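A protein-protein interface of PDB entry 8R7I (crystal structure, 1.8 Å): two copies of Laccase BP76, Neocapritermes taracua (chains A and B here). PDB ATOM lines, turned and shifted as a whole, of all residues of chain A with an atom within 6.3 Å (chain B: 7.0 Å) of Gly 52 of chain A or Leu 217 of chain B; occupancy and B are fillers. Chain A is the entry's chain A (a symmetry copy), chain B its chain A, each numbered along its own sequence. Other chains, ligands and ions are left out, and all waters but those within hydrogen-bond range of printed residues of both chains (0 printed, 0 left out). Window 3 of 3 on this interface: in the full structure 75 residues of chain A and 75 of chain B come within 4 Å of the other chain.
N of Leu 217 of chain B is in hydrogen-bond range of OE2 of Glu 77 of chain A, 3.4 Å away.
The backbone NH (N) of Gln 218 of chain B sits at hydrogen-bond distance from the side-chain carboxylate (OE2) of Glu 77 of chain A (3.0 Å).
N of Arg 219 of chain B is in hydrogen-bond range of OE1 of Glu 77 of chain A (2.8 Å).
The backbone carbonyl oxygen of Pro 214 of chain B sits at hydrogen-bond distance from the backbone NH of Val 436 of chain B, 2.8 Å away.
The guanidinium group (NE) of Arg 440 of chain B is in hydrogen-bond range of the backbone carbonyl oxygen (O) of Leu 217 of chain B (2.7 Å).
The guanidinium group (NH2) of Arg 440 of chain B is in hydrogen-bond range of the backbone carbonyl oxygen (O) of Gln 218 of chain B (2.9 Å).
Among the printed residues, merely in contact across the chains: Val 49 of chain A with Pro 214 of chain B (3.9 Å), Val 49 of chain A with Gly 215 of chain B (3.4 Å), Gly 52 of chain A with Leu 217 of chain B (3.9 Å), Pro 53 of chain A with Leu 217 of chain B (3.9 Å), Pro 53 of chain A with Phe 426 of chain B (3.4 Å), Pro 53 of chain A with Leu 442 of chain B (3.9 Å) and Glu 77 of chain A with Leu 216 of chain B (3.6 Å).
Of chain B, only Leu 217 comes within 4 Å of Gly 52 of chain A.
Of the printed residues of chain A, Leu 217 of chain B touches Gly 52, Pro 53 and Glu 77.
Of the printed residues of chain A, Pro 214 of chain B touches Val 49 (3.9 Å).
Of the printed residues of chain A, Leu 442 of chain B touches Pro 53.
The nearest residue of chain A that does not touch Leu 217 of chain B is Val 49 of chain A (6.2 Å).
Printed residues of chain A that touch a printed residue of chain B: Val 49, Gly 52, Pro 53 and Glu 77.
Hydrophobic or aromatic side chains of chain A within 4 Å of the printed part of chain B: Val 49 and Pro 53.
Hydrophobic or aromatic side chains of chain B within 4 Å of the printed part of chain A: Pro 214, Leu 216, Leu 217, Phe 426 and Leu 442.
Among the printed residues, no Asp or Glu carboxylate lies within 4 Å of a Lys or Arg side-chain nitrogen of the other chain.
No position is printed for both chains.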
ATOM      1  N   VAL A  49      -5.130  -1.462  13.094  1.00  0.00           N
ATOM      2  CA  VAL A  49      -4.079  -1.789  12.134  1.00  0.00           C
ATOM      3  C   VAL A  49      -4.578  -2.851  11.172  1.00  0.00           C
ATOM      4  O   VAL A  49      -5.423  -3.653  11.557  1.00  0.00           O
ATOM      5  CB  VAL A  49      -2.796  -2.281  12.865  1.00  0.00           C
ATOM      6  CG1 VAL A  49      -2.257  -1.209  13.776  1.00  0.00           C
ATOM      7  CG2 VAL A  49      -3.036  -3.546  13.652  1.00  0.00           C
ATOM      8  N   THR A  50      -3.966  -2.903   9.977  1.00  0.00           N
ATOM      9  CA  THR A  50      -4.018  -4.065   9.105  1.00  0.00           C
ATOM     10  C   THR A  50      -2.927  -5.040   9.595  1.00  0.00           C
ATOM     11  O   THR A  50      -1.965  -4.602  10.244  1.00  0.00           O
ATOM     12  CB  THR A  50      -3.831  -3.686   7.630  1.00  0.00           C
ATOM     13  OG1 THR A  50      -2.563  -3.054   7.493  1.00  0.00           O
ATOM     14  CG2 THR A  50      -4.943  -2.797   7.111  1.00  0.00           C
ATOM     15  N   LEU A  51      -3.120  -6.333   9.345  1.00  0.00           N
ATOM     16  CA  LEU A  51      -2.302  -7.405   9.883  1.00  0.00           C
ATOM     17  C   LEU A  51      -2.140  -7.202  11.397  1.00  0.00           C
ATOM     18  O   LEU A  51      -3.140  -7.041  12.100  1.00  0.00           O
ATOM     19  CB  LEU A  51      -1.006  -7.492   9.091  1.00  0.00           C
ATOM     20  CG  LEU A  51      -1.188  -7.774   7.579  1.00  0.00           C
ATOM     21  CD1 LEU A  51       0.145  -8.036   6.910  1.00  0.00           C
ATOM     22  CD2 LEU A  51      -2.092  -8.950   7.303  1.00  0.00           C
ATOM     23  N   GLY A  52      -0.919  -7.229  11.912  1.00  0.00           N
ATOM     24  CA  GLY A  52      -0.687  -7.050  13.343  1.00  0.00           C
ATOM     25  C   GLY A  52      -1.029  -8.293  14.164  1.00  0.00           C
ATOM     26  O   GLY A  52      -1.163  -9.394  13.624  1.00  0.00           O
ATOM     27  N   PRO A  53      -1.142  -8.125  15.486  1.00  0.00           N
ATOM     28  CA  PRO A  53      -1.238  -9.249  16.424  1.00  0.00           C
ATOM     29  C   PRO A  53      -2.431 -10.183  16.211  1.00  0.00           C
ATOM     30  O   PRO A  53      -2.318 -11.356  16.510  1.00  0.00           O
ATOM     31  CB  PRO A  53      -1.327  -8.586  17.807  1.00  0.00           C
ATOM     32  CG  PRO A  53      -0.800  -7.208  17.616  1.00  0.00           C
ATOM     33  CD  PRO A  53      -1.086  -6.822  16.164  1.00  0.00           C
ATOM     34  N   ALA A  54      -3.585  -9.685  15.750  1.00  0.00           N
ATOM     35  CA  ALA A  54      -4.746 -10.545  15.528  1.00  0.00           C
ATOM     36  C   ALA A  54      -4.615 -11.427  14.282  1.00  0.00           C
ATOM     37  O   ALA A  54      -5.442 -12.323  14.114  1.00  0.00           O
ATOM     38  CB  ALA A  54      -6.019  -9.703  15.412  1.00  0.00           C
ATOM     39  N   CYS A  55      -3.632 -11.184  13.396  1.00  0.00           N
ATOM     40  CA  CYS A  55      -3.598 -11.786  12.083  1.00  0.00           C
ATOM     41  C   CYS A  55      -2.575 -12.929  11.994  1.00  0.00           C
ATOM     42  O   CYS A  55      -2.444 -13.514  10.915  1.00  0.00           O
ATOM     43  CB  CYS A  55      -3.308 -10.745  10.992  1.00  0.00           C
ATOM     44  SG  CYS A  55      -4.703  -9.613  10.681  1.00  0.00           S
ATOM     45  N   GLY A  56      -1.838 -13.226  13.066  1.00  0.00           N
ATOM     46  CA  GLY A  56      -0.853 -14.313  13.049  1.00  0.00           C
ATOM     47  C   GLY A  56       0.026 -14.230  11.810  1.00  0.00           C
ATOM     48  O   GLY A  56       0.614 -13.158  11.556  1.00  0.00           O
ATOM     49  N   VAL A  71      -7.738  -7.746  10.172  1.00  0.00           N
ATOM     50  CA  VAL A  71      -8.052  -6.973   8.974  1.00  0.00           C
ATOM     51  C   VAL A  71      -6.920  -7.186   7.964  1.00  0.00           C
ATOM     52  O   VAL A  71      -5.814  -6.663   8.163  1.00  0.00           O
ATOM     53  CB  VAL A  71      -8.286  -5.485   9.258  1.00  0.00           C
ATOM     54  CG1 VAL A  71      -8.657  -4.729   7.993  1.00  0.00           C
ATOM     55  CG2 VAL A  71      -9.370  -5.292  10.312  1.00  0.00           C
ATOM     56  N   GLU A  77       0.844  -3.242   5.859  1.00  0.00           N
ATOM     57  CA  GLU A  77       0.626  -2.786   7.237  1.00  0.00           C
ATOM     58  C   GLU A  77       0.494  -1.273   7.285  1.00  0.00           C
ATOM     59  O   GLU A  77       1.390  -0.560   6.833  1.00  0.00           O
ATOM     60  CB  GLU A  77       1.792  -3.125   8.182  1.00  0.00           C
ATOM     61  CG  GLU A  77       1.883  -4.523   8.613  1.00  0.00           C
ATOM     62  CD  GLU A  77       3.058  -4.702   9.574  1.00  0.00           C
ATOM     63  OE1 GLU A  77       4.177  -4.564   9.081  1.00  0.00           O
ATOM     64  OE2 GLU A  77       2.812  -4.944  10.759  1.00  0.00           O
ATOM     65  N   PRO B 214      -2.132   2.050  17.000  1.00  0.00           N
ATOM     66  CA  PRO B 214      -1.314   1.278  17.939  1.00  0.00           C
ATOM     67  C   PRO B 214       0.156   1.002  17.568  1.00  0.00           C
ATOM     68  O   PRO B 214       0.943   0.706  18.459  1.00  0.00           O
ATOM     69  CB  PRO B 214      -2.048  -0.087  17.972  1.00  0.00           C
ATOM     70  CG  PRO B 214      -3.468   0.239  17.606  1.00  0.00           C
ATOM     71  CD  PRO B 214      -3.341   1.330  16.546  1.00  0.00           C
ATOM     72  N   GLY B 215       0.519   1.146  16.290  1.00  0.00           N
ATOM     73  CA  GLY B 215       1.860   0.847  15.818  1.00  0.00           C
ATOM     74  C   GLY B 215       1.878  -0.429  14.965  1.00  0.00           C
ATOM     75  O   GLY B 215       0.905  -1.209  15.037  1.00  0.00           O
ATOM     76  N   LEU B 216       2.904  -0.580  14.102  1.00  0.00           N
ATOM     77  CA  LEU B 216       2.919  -1.548  13.011  1.00  0.00           C
ATOM     78  C   LEU B 216       3.937  -2.661  13.356  1.00  0.00           C
ATOM     79  O   LEU B 216       5.143  -2.487  13.145  1.00  0.00           O
ATOM     80  CB  LEU B 216       3.286  -0.818  11.714  1.00  0.00           C
ATOM     81  CG  LEU B 216       2.382   0.382  11.356  1.00  0.00           C
ATOM     82  CD1 LEU B 216       2.765   0.925   9.985  1.00  0.00           C
ATOM     83  CD2 LEU B 216       0.913   0.011  11.363  1.00  0.00           C
ATOM     84  N   LEU B 217       3.410  -3.774  13.857  1.00  0.00           N
ATOM     85  CA  LEU B 217       4.145  -4.885  14.452  1.00  0.00           C
ATOM     86  C   LEU B 217       5.407  -5.242  13.657  1.00  0.00           C
ATOM     87  O   LEU B 217       6.482  -5.299  14.280  1.00  0.00           O
ATOM     88  CB  LEU B 217       3.215  -6.082  14.575  1.00  0.00           C
ATOM     89  CG  LEU B 217       3.783  -7.336  15.199  1.00  0.00           C
ATOM     90  CD1 LEU B 217       4.239  -7.087  16.626  1.00  0.00           C
ATOM     91  CD2 LEU B 217       2.735  -8.440  15.129  1.00  0.00           C
ATOM     92  N   GLN B 218       5.293  -5.506  12.333  1.00  0.00           N
ATOM     93  CA  GLN B 218       6.439  -6.026  11.576  1.00  0.00           C
ATOM     94  C   GLN B 218       7.283  -4.897  10.987  1.00  0.00           C
ATOM     95  O   GLN B 218       8.470  -4.823  11.314  1.00  0.00           O
ATOM     96  CB  GLN B 218       6.035  -7.051  10.505  1.00  0.00           C
ATOM     97  CG  GLN B 218       5.520  -8.355  11.094  1.00  0.00           C
ATOM     98  CD  GLN B 218       6.483  -9.048  12.045  1.00  0.00           C
ATOM     99  OE1 GLN B 218       7.703  -8.913  11.943  1.00  0.00           O
ATOM    100  NE2 GLN B 218       5.942  -9.726  13.037  1.00  0.00           N
ATOM    101  N   ARG B 219       6.721  -4.051  10.115  1.00  0.00           N
ATOM    102  CA  ARG B 219       7.561  -3.130   9.316  1.00  0.00           C
ATOM    103  C   ARG B 219       8.012  -1.886  10.096  1.00  0.00           C
ATOM    104  O   ARG B 219       9.009  -1.286   9.705  1.00  0.00           O
ATOM    105  CB  ARG B 219       6.928  -2.739   7.969  1.00  0.00           C
ATOM    106  CG  ARG B 219       5.792  -1.742   8.049  1.00  0.00           C
ATOM    107  CD  ARG B 219       5.380  -1.324   6.649  1.00  0.00           C
ATOM    108  NE  ARG B 219       4.253  -0.378   6.686  1.00  0.00           N
ATOM    109  CZ  ARG B 219       4.358   0.943   6.824  1.00  0.00           C
ATOM    110  NH1 ARG B 219       5.549   1.518   6.954  1.00  0.00           N
ATOM    111  NH2 ARG B 219       3.264   1.699   6.818  1.00  0.00           N
ATOM    112  N   LEU B 220       7.328  -1.491  11.177  1.00  0.00           N
ATOM    113  CA  LEU B 220       7.689  -0.249  11.856  1.00  0.00           C
ATOM    114  C   LEU B 220       7.106  -0.235  13.272  1.00  0.00           C
ATOM    115  O   LEU B 220       6.241   0.566  13.590  1.00  0.00           O
ATOM    116  CB  LEU B 220       7.158   0.937  11.018  1.00  0.00           C
ATOM    117  CG  LEU B 220       7.610   2.350  11.442  1.00  0.00           C
ATOM    118  CD1 LEU B 220       9.094   2.483  11.517  1.00  0.00           C
ATOM    119  CD2 LEU B 220       7.053   3.399  10.489  1.00  0.00           C
ATOM    120  N   PRO B 221       7.549  -1.150  14.160  1.00  0.00           N
ATOM    121  CA  PRO B 221       7.049  -1.154  15.522  1.00  0.00           C
ATOM    122  C   PRO B 221       7.571   0.088  16.271  1.00  0.00           C
ATOM    123  O   PRO B 221       8.633   0.588  15.993  1.00  0.00           O
ATOM    124  CB  PRO B 221       7.615  -2.446  16.112  1.00  0.00           C
ATOM    125  CG  PRO B 221       8.869  -2.707  15.292  1.00  0.00           C
ATOM    126  CD  PRO B 221       8.537  -2.204  13.904  1.00  0.00           C
ATOM    127  N   GLY B 222       6.807   0.555  17.238  1.00  0.00           N
ATOM    128  CA  GLY B 222       7.250   1.597  18.141  1.00  0.00           C
ATOM    129  C   GLY B 222       7.051   3.013  17.592  1.00  0.00           C
ATOM    130  O   GLY B 222       6.497   3.215  16.475  1.00  0.00           O
ATOM    131  N   PHE B 426      -6.658 -10.901  21.830  1.00  0.00           N
ATOM    132  CA  PHE B 426      -7.220 -10.727  20.477  1.00  0.00           C
ATOM    133  C   PHE B 426      -8.140 -11.895  20.094  1.00  0.00           C
ATOM    134  O   PHE B 426      -7.997 -12.994  20.623  1.00  0.00           O
ATOM    135  CB  PHE B 426      -6.134 -10.560  19.418  1.00  0.00           C
ATOM    136  CG  PHE B 426      -5.311  -9.309  19.619  1.00  0.00           C
ATOM    137  CD1 PHE B 426      -5.776  -8.075  19.192  1.00  0.00           C
ATOM    138  CD2 PHE B 426      -4.103  -9.364  20.305  1.00  0.00           C
ATOM    139  CE1 PHE B 426      -5.052  -6.913  19.439  1.00  0.00           C
ATOM    140  CE2 PHE B 426      -3.373  -8.214  20.535  1.00  0.00           C
ATOM    141  CZ  PHE B 426      -3.854  -6.983  20.121  1.00  0.00           C
ATOM    142  N   PHE B 434      -4.007  -1.251  23.265  1.00  0.00           N
ATOM    143  CA  PHE B 434      -2.620  -1.679  23.216  1.00  0.00           C
ATOM    144  C   PHE B 434      -1.814  -0.753  22.308  1.00  0.00           C
ATOM    145  O   PHE B 434      -2.388  -0.073  21.433  1.00  0.00           O
ATOM    146  CB  PHE B 434      -2.498  -3.120  22.692  1.00  0.00           C
ATOM    147  CG  PHE B 434      -2.783  -3.259  21.213  1.00  0.00           C
ATOM    148  CD1 PHE B 434      -4.077  -3.158  20.725  1.00  0.00           C
ATOM    149  CD2 PHE B 434      -1.746  -3.471  20.324  1.00  0.00           C
ATOM    150  CE1 PHE B 434      -4.335  -3.272  19.365  1.00  0.00           C
ATOM    151  CE2 PHE B 434      -1.999  -3.593  18.962  1.00  0.00           C
ATOM    152  CZ  PHE B 434      -3.290  -3.501  18.489  1.00  0.00           C
ATOM    153  N   VAL B 436       2.243  -0.997  20.248  1.00  0.00           N
ATOM    154  CA  VAL B 436       3.368  -1.862  19.892  1.00  0.00           C
ATOM    155  C   VAL B 436       4.662  -1.054  20.048  1.00  0.00           C
ATOM    156  O   VAL B 436       4.845  -0.054  19.340  1.00  0.00           O
ATOM    157  CB  VAL B 436       3.251  -2.372  18.435  1.00  0.00           C
ATOM    158  CG1 VAL B 436       4.381  -3.337  18.087  1.00  0.00           C
ATOM    159  CG2 VAL B 436       1.895  -3.006  18.162  1.00  0.00           C
ATOM    160  N   VAL B 437       5.553  -1.512  20.938  1.00  0.00           N
ATOM    161  CA  VAL B 437       6.801  -0.806  21.205  1.00  0.00           C
ATOM    162  C   VAL B 437       7.882  -1.356  20.258  1.00  0.00           C
ATOM    163  O   VAL B 437       7.652  -2.369  19.602  1.00  0.00           O
ATOM    164  CB  VAL B 437       7.160  -0.877  22.704  1.00  0.00           C
ATOM    165  CG1 VAL B 437       6.063  -0.214  23.527  1.00  0.00           C
ATOM    166  CG2 VAL B 437       7.422  -2.275  23.200  1.00  0.00           C
ATOM    167  N   PRO B 438       9.061  -0.724  20.134  1.00  0.00           N
ATOM    168  CA  PRO B 438      10.070  -1.166  19.167  1.00  0.00           C
ATOM    169  C   PRO B 438      10.480  -2.633  19.250  1.00  0.00           C
ATOM    170  O   PRO B 438      10.709  -3.197  18.196  1.00  0.00           O
ATOM    171  CB  PRO B 438      11.251  -0.217  19.396  1.00  0.00           C
ATOM    172  CG  PRO B 438      10.610   1.044  19.970  1.00  0.00           C
ATOM    173  CD  PRO B 438       9.475   0.522  20.839  1.00  0.00           C
ATOM    174  N   ASP B 439      10.485  -3.247  20.441  1.00  0.00           N
ATOM    175  CA  ASP B 439      10.912  -4.663  20.554  1.00  0.00           C
ATOM    176  C   ASP B 439       9.711  -5.592  20.336  1.00  0.00           C
ATOM    177  O   ASP B 439       9.842  -6.800  20.488  1.00  0.00           O
ATOM    178  CB  ASP B 439      11.601  -4.938  21.900  1.00  0.00           C
ATOM    179  CG  ASP B 439      10.704  -4.830  23.115  1.00  0.00           C
ATOM    180  OD1 ASP B 439       9.443  -4.686  22.960  1.00  0.00           O
ATOM    181  OD2 ASP B 439      11.254  -4.852  24.227  1.00  0.00           O
ATOM    182  N   ARG B 440       8.538  -5.034  19.930  1.00  0.00           N
ATOM    183  CA  ARG B 440       7.335  -5.760  19.508  1.00  0.00           C
ATOM    184  C   ARG B 440       6.526  -6.296  20.697  1.00  0.00           C
ATOM    185  O   ARG B 440       5.515  -7.001  20.490  1.00  0.00           O
ATOM    186  CB  ARG B 440       7.615  -6.855  18.467  1.00  0.00           C
ATOM    187  CG  ARG B 440       8.221  -6.306  17.188  1.00  0.00           C
ATOM    188  CD  ARG B 440       8.270  -7.390  16.094  1.00  0.00           C
ATOM    189  NE  ARG B 440       8.669  -6.796  14.859  1.00  0.00           N
ATOM    190  CZ  ARG B 440       9.899  -6.828  14.356  1.00  0.00           C
ATOM    191  NH1 ARG B 440      10.858  -7.495  14.996  1.00  0.00           N
ATOM    192  NH2 ARG B 440      10.164  -6.242  13.197  1.00  0.00           N
ATOM    193  N   ASN B 441       6.869  -5.899  21.922  1.00  0.00           N
ATOM    194  CA  ASN B 441       5.981  -6.106  23.068  1.00  0.00           C
ATOM    195  C   ASN B 441       4.666  -5.328  22.842  1.00  0.00           C
ATOM    196  O   ASN B 441       4.675  -4.291  22.189  1.00  0.00           O
ATOM    197  CB  ASN B 441       6.624  -5.709  24.390  1.00  0.00           C
ATOM    198  CG  ASN B 441       7.611  -6.748  24.919  1.00  0.00           C
ATOM    199  OD1 ASN B 441       7.426  -7.930  24.707  1.00  0.00           O
ATOM    200  ND2 ASN B 441       8.585  -6.299  25.697  1.00  0.00           N
ATOM    201  N   LEU B 442       3.551  -5.841  23.373  1.00  0.00           N
ATOM    202  CA  LEU B 442       2.220  -5.266  23.240  1.00  0.00           C
ATOM    203  C   LEU B 442       1.811  -4.767  24.624  1.00  0.00           C
ATOM    204  O   LEU B 442       1.642  -5.600  25.539  1.00  0.00           O
ATOM    205  CB  LEU B 442       1.233  -6.313  22.724  1.00  0.00           C
ATOM    206  CG  LEU B 442       1.641  -7.065  21.462  1.00  0.00           C
ATOM    207  CD1 LEU B 442       0.582  -8.081  21.124  1.00  0.00           C
ATOM    208  CD2 LEU B 442       1.902  -6.119  20.288  1.00  0.00           C
